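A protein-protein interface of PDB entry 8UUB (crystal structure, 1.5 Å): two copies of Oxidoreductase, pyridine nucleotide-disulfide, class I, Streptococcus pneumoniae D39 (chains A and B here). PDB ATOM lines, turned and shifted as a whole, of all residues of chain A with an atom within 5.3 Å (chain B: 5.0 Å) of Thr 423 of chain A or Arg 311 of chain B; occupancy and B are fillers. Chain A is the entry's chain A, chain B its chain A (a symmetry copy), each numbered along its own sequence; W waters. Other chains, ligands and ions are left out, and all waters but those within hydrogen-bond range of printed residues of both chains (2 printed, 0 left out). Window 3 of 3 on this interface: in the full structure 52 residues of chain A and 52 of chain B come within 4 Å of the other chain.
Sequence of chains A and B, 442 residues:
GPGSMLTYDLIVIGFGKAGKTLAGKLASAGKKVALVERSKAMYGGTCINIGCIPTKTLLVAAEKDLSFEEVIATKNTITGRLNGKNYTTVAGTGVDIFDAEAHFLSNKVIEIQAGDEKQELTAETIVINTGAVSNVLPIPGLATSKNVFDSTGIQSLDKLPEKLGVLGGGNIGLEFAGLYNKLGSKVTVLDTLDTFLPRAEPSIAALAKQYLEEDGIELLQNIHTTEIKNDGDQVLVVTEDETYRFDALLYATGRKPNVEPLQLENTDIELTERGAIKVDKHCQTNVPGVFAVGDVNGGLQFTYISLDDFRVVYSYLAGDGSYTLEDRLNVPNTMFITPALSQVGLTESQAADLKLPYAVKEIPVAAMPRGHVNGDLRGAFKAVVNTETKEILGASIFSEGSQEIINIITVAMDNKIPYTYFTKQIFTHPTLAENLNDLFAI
The guanidinium group (NE) of Arg 311 of chain B lies within hydrogen-bond range of the backbone carbonyl oxygen (O) of Thr 423 of chain A (3.2 Å).
The backbone carbonyl oxygen (O) of Gln 425 of chain A lies within hydrogen-bond range of the side-chain amide nitrogen (ND2) of Asn 437 of chain A (2.9 Å). OG1 of Thr 423 of chain A lies within hydrogen-bond range of O of Thr 420 of chain A (2.7 Å). O of Phe 422 of chain A sits at hydrogen-bond distance from ND2 of Asn 437 of chain A (2.8 Å). OD2 of Asp 308 of chain B sits at hydrogen-bond distance from OH of Tyr 323 of chain B, at 2.6 Å. The guanidinium group (NH1) of Arg 311 of chain B is in salt-bridge range of the side-chain carboxylate (OD1) of Asp 308 of chain B, at 2.8 Å.
Water W1 lies within hydrogen-bond range of OD1 of Asp 308 of chain B, O of Lys 424 of chain A and OH of Tyr 323 of chain B. Water W2 bridges the guanidinium group of Arg 311 of chain B (3.2 Å) and the backbone carbonyl oxygen of Thr 423 of chain A (3.2 Å).
Among the printed residues, merely in contact across the chains: Ile 426 of chain A with Tyr 304 of chain B (3.3 Å), Asn 437 of chain A with Arg 311 of chain B (3.5 Å), Gln 425 of chain A with Arg 311 of chain B (3.7 Å), Ile 426 of chain A with Asp 308 of chain B (3.8 Å), Lys 424 of chain A with Arg 311 of chain B (3.8 Å) and Asn 437 of chain A with Leu 307 of chain B (3.9 Å).
Thr 423 of chain A touches just one residue of chain B: Arg 311. Printed residues of chain B within 4 Å of Lys 424 of chain A: Arg 311 (3.8 Å). Of the printed residues of chain B, Gln 425 of chain A touches Arg 311. Printed residues of chain A within 4 Å of Leu 307 of chain B: Asn 437 (3.9 Å). Phe 310 of chain B touches none of the printed residues of chain A. Tyr 323 of chain B touches none of the printed residues of chain A. The nearest residue of chain A that does not touch Arg 311 of chain B is Ile 426 of chain A (4.2 Å).
No position is printed for both chains. Of the 7 pairs that touch across the chains among the printed residues, none has its exchanged pair printed and touching as well.
Printed residues of chain B that touch a printed residue of chain A: Tyr 304, Leu 307, Asp 308 and Arg 311. Hydrophobic or aromatic side chains of chain B that line the printed part of chain A: Tyr 304 and Leu 307. Of the 12 printed residues of chain A, 5 touch a printed residue of chain B.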
ATOM      1  N   TYR A 419      15.707 -15.580  -2.818  1.00  0.00           N
ATOM      2  CA  TYR A 419      16.640 -14.472  -2.650  1.00  0.00           C
ATOM      3  C   TYR A 419      17.344 -14.164  -3.960  1.00  0.00           C
ATOM      4  O   TYR A 419      17.783 -13.027  -4.179  1.00  0.00           O
ATOM      5  CB  TYR A 419      17.611 -14.746  -1.500  1.00  0.00           C
ATOM      6  CG  TYR A 419      18.676 -15.774  -1.801  1.00  0.00           C
ATOM      7  CD1 TYR A 419      19.827 -15.407  -2.477  1.00  0.00           C
ATOM      8  CD2 TYR A 419      18.607 -17.027  -1.218  1.00  0.00           C
ATOM      9  CE1 TYR A 419      20.852 -16.304  -2.702  1.00  0.00           C
ATOM     10  CE2 TYR A 419      19.625 -17.950  -1.427  1.00  0.00           C
ATOM     11  CZ  TYR A 419      20.732 -17.562  -2.164  1.00  0.00           C
ATOM     12  OH  TYR A 419      21.756 -18.454  -2.381  1.00  0.00           O
ATOM     13  N   THR A 420      17.487 -15.175  -4.825  1.00  0.00           N
ATOM     14  CA  THR A 420      18.205 -14.977  -6.089  1.00  0.00           C
ATOM     15  C   THR A 420      17.472 -13.986  -6.988  1.00  0.00           C
ATOM     16  O   THR A 420      18.059 -13.399  -7.900  1.00  0.00           O
ATOM     17  CB  THR A 420      18.333 -16.332  -6.804  1.00  0.00           C
ATOM     18  OG1 THR A 420      17.054 -16.964  -6.840  1.00  0.00           O
ATOM     19  CG2 THR A 420      19.235 -17.267  -6.027  1.00  0.00           C
ATOM     20  N   TYR A 421      16.155 -13.728  -6.756  1.00  0.00           N
ATOM     21  CA  TYR A 421      15.460 -12.729  -7.563  1.00  0.00           C
ATOM     22  C   TYR A 421      16.171 -11.366  -7.476  1.00  0.00           C
ATOM     23  O   TYR A 421      16.233 -10.624  -8.467  1.00  0.00           O
ATOM     24  CB  TYR A 421      13.983 -12.586  -7.078  1.00  0.00           C
ATOM     25  CG  TYR A 421      13.353 -11.314  -7.595  1.00  0.00           C
ATOM     26  CD1 TYR A 421      12.971 -11.164  -8.911  1.00  0.00           C
ATOM     27  CD2 TYR A 421      13.228 -10.192  -6.758  1.00  0.00           C
ATOM     28  CE1 TYR A 421      12.543  -9.964  -9.483  1.00  0.00           C
ATOM     29  CE2 TYR A 421      12.771  -8.997  -7.278  1.00  0.00           C
ATOM     30  CZ  TYR A 421      12.464  -8.852  -8.619  1.00  0.00           C
ATOM     31  OH  TYR A 421      12.012  -7.671  -9.089  1.00  0.00           O
ATOM     32  N   PHE A 422      16.687 -11.082  -6.299  1.00  0.00           N
ATOM     33  CA  PHE A 422      17.274  -9.746  -6.144  1.00  0.00           C
ATOM     34  C   PHE A 422      18.555  -9.585  -6.958  1.00  0.00           C
ATOM     35  O   PHE A 422      18.969  -8.452  -7.199  1.00  0.00           O
ATOM     36  CB  PHE A 422      17.476  -9.364  -4.675  1.00  0.00           C
ATOM     37  CG  PHE A 422      16.210  -8.880  -3.995  1.00  0.00           C
ATOM     38  CD1 PHE A 422      15.438  -7.896  -4.562  1.00  0.00           C
ATOM     39  CD2 PHE A 422      15.832  -9.464  -2.799  1.00  0.00           C
ATOM     40  CE1 PHE A 422      14.291  -7.434  -3.905  1.00  0.00           C
ATOM     41  CE2 PHE A 422      14.682  -8.994  -2.136  1.00  0.00           C
ATOM     42  CZ  PHE A 422      13.886  -8.008  -2.720  1.00  0.00           C
ATOM     43  N   THR A 423      19.180 -10.702  -7.384  1.00  0.00           N
ATOM     44  CA  THR A 423      20.321 -10.594  -8.300  1.00  0.00           C
ATOM     45  C   THR A 423      19.894 -10.255  -9.710  1.00  0.00           C
ATOM     46  O   THR A 423      20.767  -9.944 -10.558  1.00  0.00           O
ATOM     47  CB  THR A 423      21.239 -11.838  -8.269  1.00  0.00           C
ATOM     48  OG1 THR A 423      20.559 -12.913  -8.919  1.00  0.00           O
ATOM     49  CG2 THR A 423      21.660 -12.182  -6.859  1.00  0.00           C
ATOM     50  N   LYS A 424      18.606 -10.376 -10.027  1.00  0.00           N
ATOM     51  CA  LYS A 424      18.092 -10.182 -11.364  1.00  0.00           C
ATOM     52  C   LYS A 424      17.249  -8.925 -11.544  1.00  0.00           C
ATOM     53  O   LYS A 424      17.034  -8.465 -12.654  1.00  0.00           O
ATOM     54  CB  LYS A 424      17.196 -11.383 -11.725  1.00  0.00           C
ATOM     55  CG  LYS A 424      17.992 -12.684 -11.795  1.00  0.00           C
ATOM     56  CD  LYS A 424      17.082 -13.906 -11.789  1.00  0.00           C
ATOM     57  CE  LYS A 424      17.964 -15.129 -11.624  1.00  0.00           C
ATOM     58  NZ  LYS A 424      17.189 -16.396 -11.562  1.00  0.00           N
ATOM     59  N   GLN A 425      16.743  -8.384 -10.405  1.00  0.00           N
ATOM     60  CA  GLN A 425      15.897  -7.194 -10.479  1.00  0.00           C
ATOM     61  C   GLN A 425      16.680  -6.049 -11.144  1.00  0.00           C
ATOM     62  O   GLN A 425      17.899  -5.835 -10.869  1.00  0.00           O
ATOM     63  CB  GLN A 425      15.472  -6.824  -9.044  1.00  0.00           C
ATOM     64  CG  GLN A 425      14.662  -5.507  -9.014  1.00  0.00           C
ATOM     65  CD  GLN A 425      13.934  -5.269  -7.695  1.00  0.00           C
ATOM     66  OE1 GLN A 425      14.066  -6.045  -6.745  1.00  0.00           O
ATOM     67  NE2 GLN A 425      13.273  -4.081  -7.643  1.00  0.00           N
ATOM     68  N   ILE A 426      15.978  -5.293 -11.975  1.00  0.00           N
ATOM     69  CA  ILE A 426      16.526  -4.110 -12.633  1.00  0.00           C
ATOM     70  C   ILE A 426      16.145  -2.897 -11.752  1.00  0.00           C
ATOM     71  O   ILE A 426      14.968  -2.479 -11.737  1.00  0.00           O
ATOM     72  CB  ILE A 426      16.012  -3.989 -14.087  1.00  0.00           C
ATOM     73  CG1 ILE A 426      16.413  -5.263 -14.866  1.00  0.00           C
ATOM     74  CG2 ILE A 426      16.527  -2.681 -14.745  1.00  0.00           C
ATOM     75  CD1 ILE A 426      15.805  -5.300 -16.255  1.00  0.00           C
ATOM     76  N   LEU A 436      21.317  -4.178  -3.625  1.00  0.00           N
ATOM     77  CA  LEU A 436      20.717  -5.480  -3.358  1.00  0.00           C
ATOM     78  C   LEU A 436      21.072  -6.493  -4.468  1.00  0.00           C
ATOM     79  O   LEU A 436      21.091  -7.699  -4.197  1.00  0.00           O
ATOM     80  CB  LEU A 436      19.187  -5.358  -3.224  1.00  0.00           C
ATOM     81  CG  LEU A 436      18.766  -4.471  -2.038  1.00  0.00           C
ATOM     82  CD1 LEU A 436      17.224  -4.397  -2.046  1.00  0.00           C
ATOM     83  CD2 LEU A 436      19.304  -4.989  -0.704  1.00  0.00           C
ATOM     84  N   ASN A 437      21.379  -6.013  -5.712  1.00  0.00           N
ATOM     85  CA  ASN A 437      21.834  -6.972  -6.724  1.00  0.00           C
ATOM     86  C   ASN A 437      23.067  -7.728  -6.242  1.00  0.00           C
ATOM     87  O   ASN A 437      23.204  -8.904  -6.640  1.00  0.00           O
ATOM     88  CB  ASN A 437      22.205  -6.225  -8.003  1.00  0.00           C
ATOM     89  CG  ASN A 437      21.095  -5.783  -8.944  1.00  0.00           C
ATOM     90  OD1 ASN A 437      21.331  -4.816  -9.698  1.00  0.00           O
ATOM     91  ND2 ASN A 437      19.942  -6.478  -8.982  1.00  0.00           N
ATOM     92  N   PHE A 440      22.621  -9.985  -2.554  1.00  0.00           N
ATOM     93  CA  PHE A 440      22.013 -11.299  -2.652  1.00  0.00           C
ATOM     94  C   PHE A 440      22.720 -12.258  -3.612  1.00  0.00           C
ATOM     95  O   PHE A 440      22.199 -13.354  -3.868  1.00  0.00           O
ATOM     96  CB  PHE A 440      20.520 -11.189  -2.968  1.00  0.00           C
ATOM     97  CG  PHE A 440      19.746 -10.704  -1.761  1.00  0.00           C
ATOM     98  CD1 PHE A 440      19.480 -11.596  -0.728  1.00  0.00           C
ATOM     99  CD2 PHE A 440      19.290  -9.395  -1.638  1.00  0.00           C
ATOM    100  CE1 PHE A 440      18.767 -11.201   0.412  1.00  0.00           C
ATOM    101  CE2 PHE A 440      18.555  -8.992  -0.506  1.00  0.00           C
ATOM    102  CZ  PHE A 440      18.315  -9.881   0.529  1.00  0.00           C
ATOM    103  N   ALA A 441      23.912 -11.856  -4.072  1.00  0.00           N
ATOM    104  CA  ALA A 441      24.707 -12.799  -4.881  1.00  0.00           C
ATOM    105  C   ALA A 441      25.591 -13.577  -3.918  1.00  0.00           C
ATOM    106  O   ALA A 441      26.761 -13.223  -3.685  1.00  0.00           O
ATOM    107  CB  ALA A 441      25.526 -11.991  -5.869  1.00  0.00           C
ATOM    108  N   TYR B 304      21.544   0.444 -15.896  1.00  0.00           N
ATOM    109  CA  TYR B 304      20.976  -0.811 -15.462  1.00  0.00           C
ATOM    110  C   TYR B 304      20.468  -1.659 -16.649  1.00  0.00           C
ATOM    111  O   TYR B 304      20.363  -2.893 -16.451  1.00  0.00           O
ATOM    112  CB  TYR B 304      19.861  -0.560 -14.422  1.00  0.00           C
ATOM    113  CG  TYR B 304      18.904   0.564 -14.698  1.00  0.00           C
ATOM    114  CD1 TYR B 304      17.721   0.371 -15.432  1.00  0.00           C
ATOM    115  CD2 TYR B 304      19.177   1.840 -14.198  1.00  0.00           C
ATOM    116  CE1 TYR B 304      16.828   1.420 -15.592  1.00  0.00           C
ATOM    117  CE2 TYR B 304      18.300   2.896 -14.408  1.00  0.00           C
ATOM    118  CZ  TYR B 304      17.104   2.665 -15.058  1.00  0.00           C
ATOM    119  OH  TYR B 304      16.184   3.652 -15.205  1.00  0.00           O
ATOM    120  N   LEU B 307      23.724  -3.272 -17.672  1.00  0.00           N
ATOM    121  CA  LEU B 307      23.998  -4.382 -16.754  1.00  0.00           C
ATOM    122  C   LEU B 307      23.156  -5.607 -17.173  1.00  0.00           C
ATOM    123  O   LEU B 307      23.649  -6.726 -17.114  1.00  0.00           O
ATOM    124  CB  LEU B 307      23.731  -3.915 -15.310  1.00  0.00           C
ATOM    125  CG  LEU B 307      23.876  -5.027 -14.284  1.00  0.00           C
ATOM    126  CD1 LEU B 307      25.282  -5.654 -14.283  1.00  0.00           C
ATOM    127  CD2 LEU B 307      23.553  -4.490 -12.880  1.00  0.00           C
ATOM    128  N   ASP B 308      21.877  -5.393 -17.489  1.00  0.00           N
ATOM    129  CA  ASP B 308      21.055  -6.547 -17.852  1.00  0.00           C
ATOM    130  C   ASP B 308      21.509  -7.168 -19.180  1.00  0.00           C
ATOM    131  O   ASP B 308      21.325  -8.385 -19.310  1.00  0.00           O
ATOM    132  CB  ASP B 308      19.575  -6.154 -17.856  1.00  0.00           C
ATOM    133  CG  ASP B 308      18.698  -7.391 -17.679  1.00  0.00           C
ATOM    134  OD1 ASP B 308      18.859  -8.122 -16.680  1.00  0.00           O
ATOM    135  OD2 ASP B 308      17.966  -7.664 -18.681  1.00  0.00           O
ATOM    136  N   ASP B 309      22.105  -6.371 -20.072  1.00  0.00           N
ATOM    137  CA  ASP B 309      22.666  -7.000 -21.293  1.00  0.00           C
ATOM    138  C   ASP B 309      23.810  -7.928 -20.906  1.00  0.00           C
ATOM    139  O   ASP B 309      24.007  -9.001 -21.538  1.00  0.00           O
ATOM    140  CB  ASP B 309      23.199  -5.981 -22.293  1.00  0.00           C
ATOM    141  CG  ASP B 309      22.166  -5.303 -23.132  1.00  0.00           C
ATOM    142  OD1 ASP B 309      20.926  -5.692 -22.996  1.00  0.00           O
ATOM    143  OD2 ASP B 309      22.505  -4.439 -23.944  1.00  0.00           O
ATOM    144  N   PHE B 310      24.601  -7.630 -19.855  1.00  0.00           N
ATOM    145  CA  PHE B 310      25.576  -8.587 -19.376  1.00  0.00           C
ATOM    146  C   PHE B 310      24.852  -9.888 -18.993  1.00  0.00           C
ATOM    147  O   PHE B 310      25.359 -10.989 -19.264  1.00  0.00           O
ATOM    148  CB  PHE B 310      26.370  -8.009 -18.172  1.00  0.00           C
ATOM    149  CG  PHE B 310      26.836  -9.083 -17.235  1.00  0.00           C
ATOM    150  CD1 PHE B 310      27.959  -9.876 -17.512  1.00  0.00           C
ATOM    151  CD2 PHE B 310      26.080  -9.383 -16.078  1.00  0.00           C
ATOM    152  CE1 PHE B 310      28.395 -10.896 -16.670  1.00  0.00           C
ATOM    153  CE2 PHE B 310      26.494 -10.430 -15.274  1.00  0.00           C
ATOM    154  CZ  PHE B 310      27.609 -11.180 -15.542  1.00  0.00           C
ATOM    155  N   ARG B 311      23.690  -9.793 -18.304  1.00  0.00           N
ATOM    156  CA  ARG B 311      23.021 -11.038 -17.899  1.00  0.00           C
ATOM    157  C   ARG B 311      22.634 -11.882 -19.134  1.00  0.00           C
ATOM    158  O   ARG B 311      22.767 -13.108 -19.106  1.00  0.00           O
ATOM    159  CB  ARG B 311      21.772 -10.730 -17.032  1.00  0.00           C
ATOM    160  CG  ARG B 311      22.128  -9.989 -15.746  1.00  0.00           C
ATOM    161  CD  ARG B 311      20.881  -9.836 -14.873  1.00  0.00           C
ATOM    162  NE  ARG B 311      21.109  -9.043 -13.657  1.00  0.00           N
ATOM    163  CZ  ARG B 311      20.771  -7.767 -13.493  1.00  0.00           C
ATOM    164  NH1 ARG B 311      20.155  -7.121 -14.461  1.00  0.00           N
ATOM    165  NH2 ARG B 311      21.075  -7.117 -12.353  1.00  0.00           N
ATOM    166  N   VAL B 312      22.186 -11.213 -20.174  1.00  0.00           N
ATOM    167  CA  VAL B 312      21.806 -11.902 -21.425  1.00  0.00           C
ATOM    168  C   VAL B 312      23.027 -12.568 -22.066  1.00  0.00           C
ATOM    169  O   VAL B 312      23.006 -13.780 -22.414  1.00  0.00           O
ATOM    170  CB  VAL B 312      21.202 -10.902 -22.412  1.00  0.00           C
ATOM    171  CG1 VAL B 312      21.049 -11.564 -23.815  1.00  0.00           C
ATOM    172  CG2 VAL B 312      19.835 -10.414 -21.943  1.00  0.00           C
ATOM    173  N   VAL B 313      24.127 -11.803 -22.209  1.00  0.00           N
ATOM    174  CA  VAL B 313      25.273 -12.378 -22.920  1.00  0.00           C
ATOM    175  C   VAL B 313      25.872 -13.488 -22.062  1.00  0.00           C
ATOM    176  O   VAL B 313      26.323 -14.526 -22.562  1.00  0.00           O
ATOM    177  CB  VAL B 313      26.293 -11.284 -23.280  1.00  0.00           C
ATOM    178  CG1 VAL B 313      27.563 -11.928 -23.820  1.00  0.00           C
ATOM    179  CG2 VAL B 313      25.680 -10.384 -24.323  1.00  0.00           C
ATOM    180  N   TYR B 314      25.972 -13.294 -20.748  1.00  0.00           N
ATOM    181  CA  TYR B 314      26.536 -14.311 -19.871  1.00  0.00           C
ATOM    182  C   TYR B 314      25.665 -15.583 -19.915  1.00  0.00           C
ATOM    183  O   TYR B 314      26.192 -16.692 -19.975  1.00  0.00           O
ATOM    184  CB  TYR B 314      26.674 -13.780 -18.430  1.00  0.00           C
ATOM    185  CG  TYR B 314      27.407 -14.746 -17.539  1.00  0.00           C
ATOM    186  CD1 TYR B 314      28.783 -14.893 -17.633  1.00  0.00           C
ATOM    187  CD2 TYR B 314      26.712 -15.596 -16.678  1.00  0.00           C
ATOM    188  CE1 TYR B 314      29.491 -15.774 -16.825  1.00  0.00           C
ATOM    189  CE2 TYR B 314      27.402 -16.545 -15.931  1.00  0.00           C
ATOM    190  CZ  TYR B 314      28.784 -16.585 -15.957  1.00  0.00           C
ATOM    191  OH  TYR B 314      29.476 -17.515 -15.215  1.00  0.00           O
ATOM    192  N   SER B 315      24.341 -15.422 -19.974  1.00  0.00           N
ATOM    193  CA  SER B 315      23.462 -16.589 -20.099  1.00  0.00           C
ATOM    194  C   SER B 315      23.831 -17.384 -21.350  1.00  0.00           C
ATOM    195  O   SER B 315      23.934 -18.618 -21.262  1.00  0.00           O
ATOM    196  CB  SER B 315      22.019 -16.148 -20.146  1.00  0.00           C
ATOM    197  OG  SER B 315      21.142 -17.294 -20.315  1.00  0.00           O
ATOM    198  N   TYR B 323      18.099 -16.928 -20.572  1.00  0.00           N
ATOM    199  CA  TYR B 323      17.640 -15.560 -20.317  1.00  0.00           C
ATOM    200  C   TYR B 323      18.029 -14.694 -21.505  1.00  0.00           C
ATOM    201  O   TYR B 323      19.224 -14.559 -21.790  1.00  0.00           O
ATOM    202  CB  TYR B 323      18.277 -14.948 -19.051  1.00  0.00           C
ATOM    203  CG  TYR B 323      17.763 -13.550 -18.782  1.00  0.00           C
ATOM    204  CD1 TYR B 323      16.445 -13.298 -18.431  1.00  0.00           C
ATOM    205  CD2 TYR B 323      18.599 -12.435 -18.922  1.00  0.00           C
ATOM    206  CE1 TYR B 323      15.974 -12.001 -18.284  1.00  0.00           C
ATOM    207  CE2 TYR B 323      18.176 -11.130 -18.708  1.00  0.00           C
ATOM    208  CZ  TYR B 323      16.846 -10.907 -18.374  1.00  0.00           C
ATOM    209  OH  TYR B 323      16.316  -9.674 -18.232  1.00  0.00           O
HETATM  210  O   HOH W   1      17.398  -9.759 -15.118  1.00  0.00           O
HETATM  211  O   HOH W   2      23.030 -11.207 -12.377  1.00  0.00           O
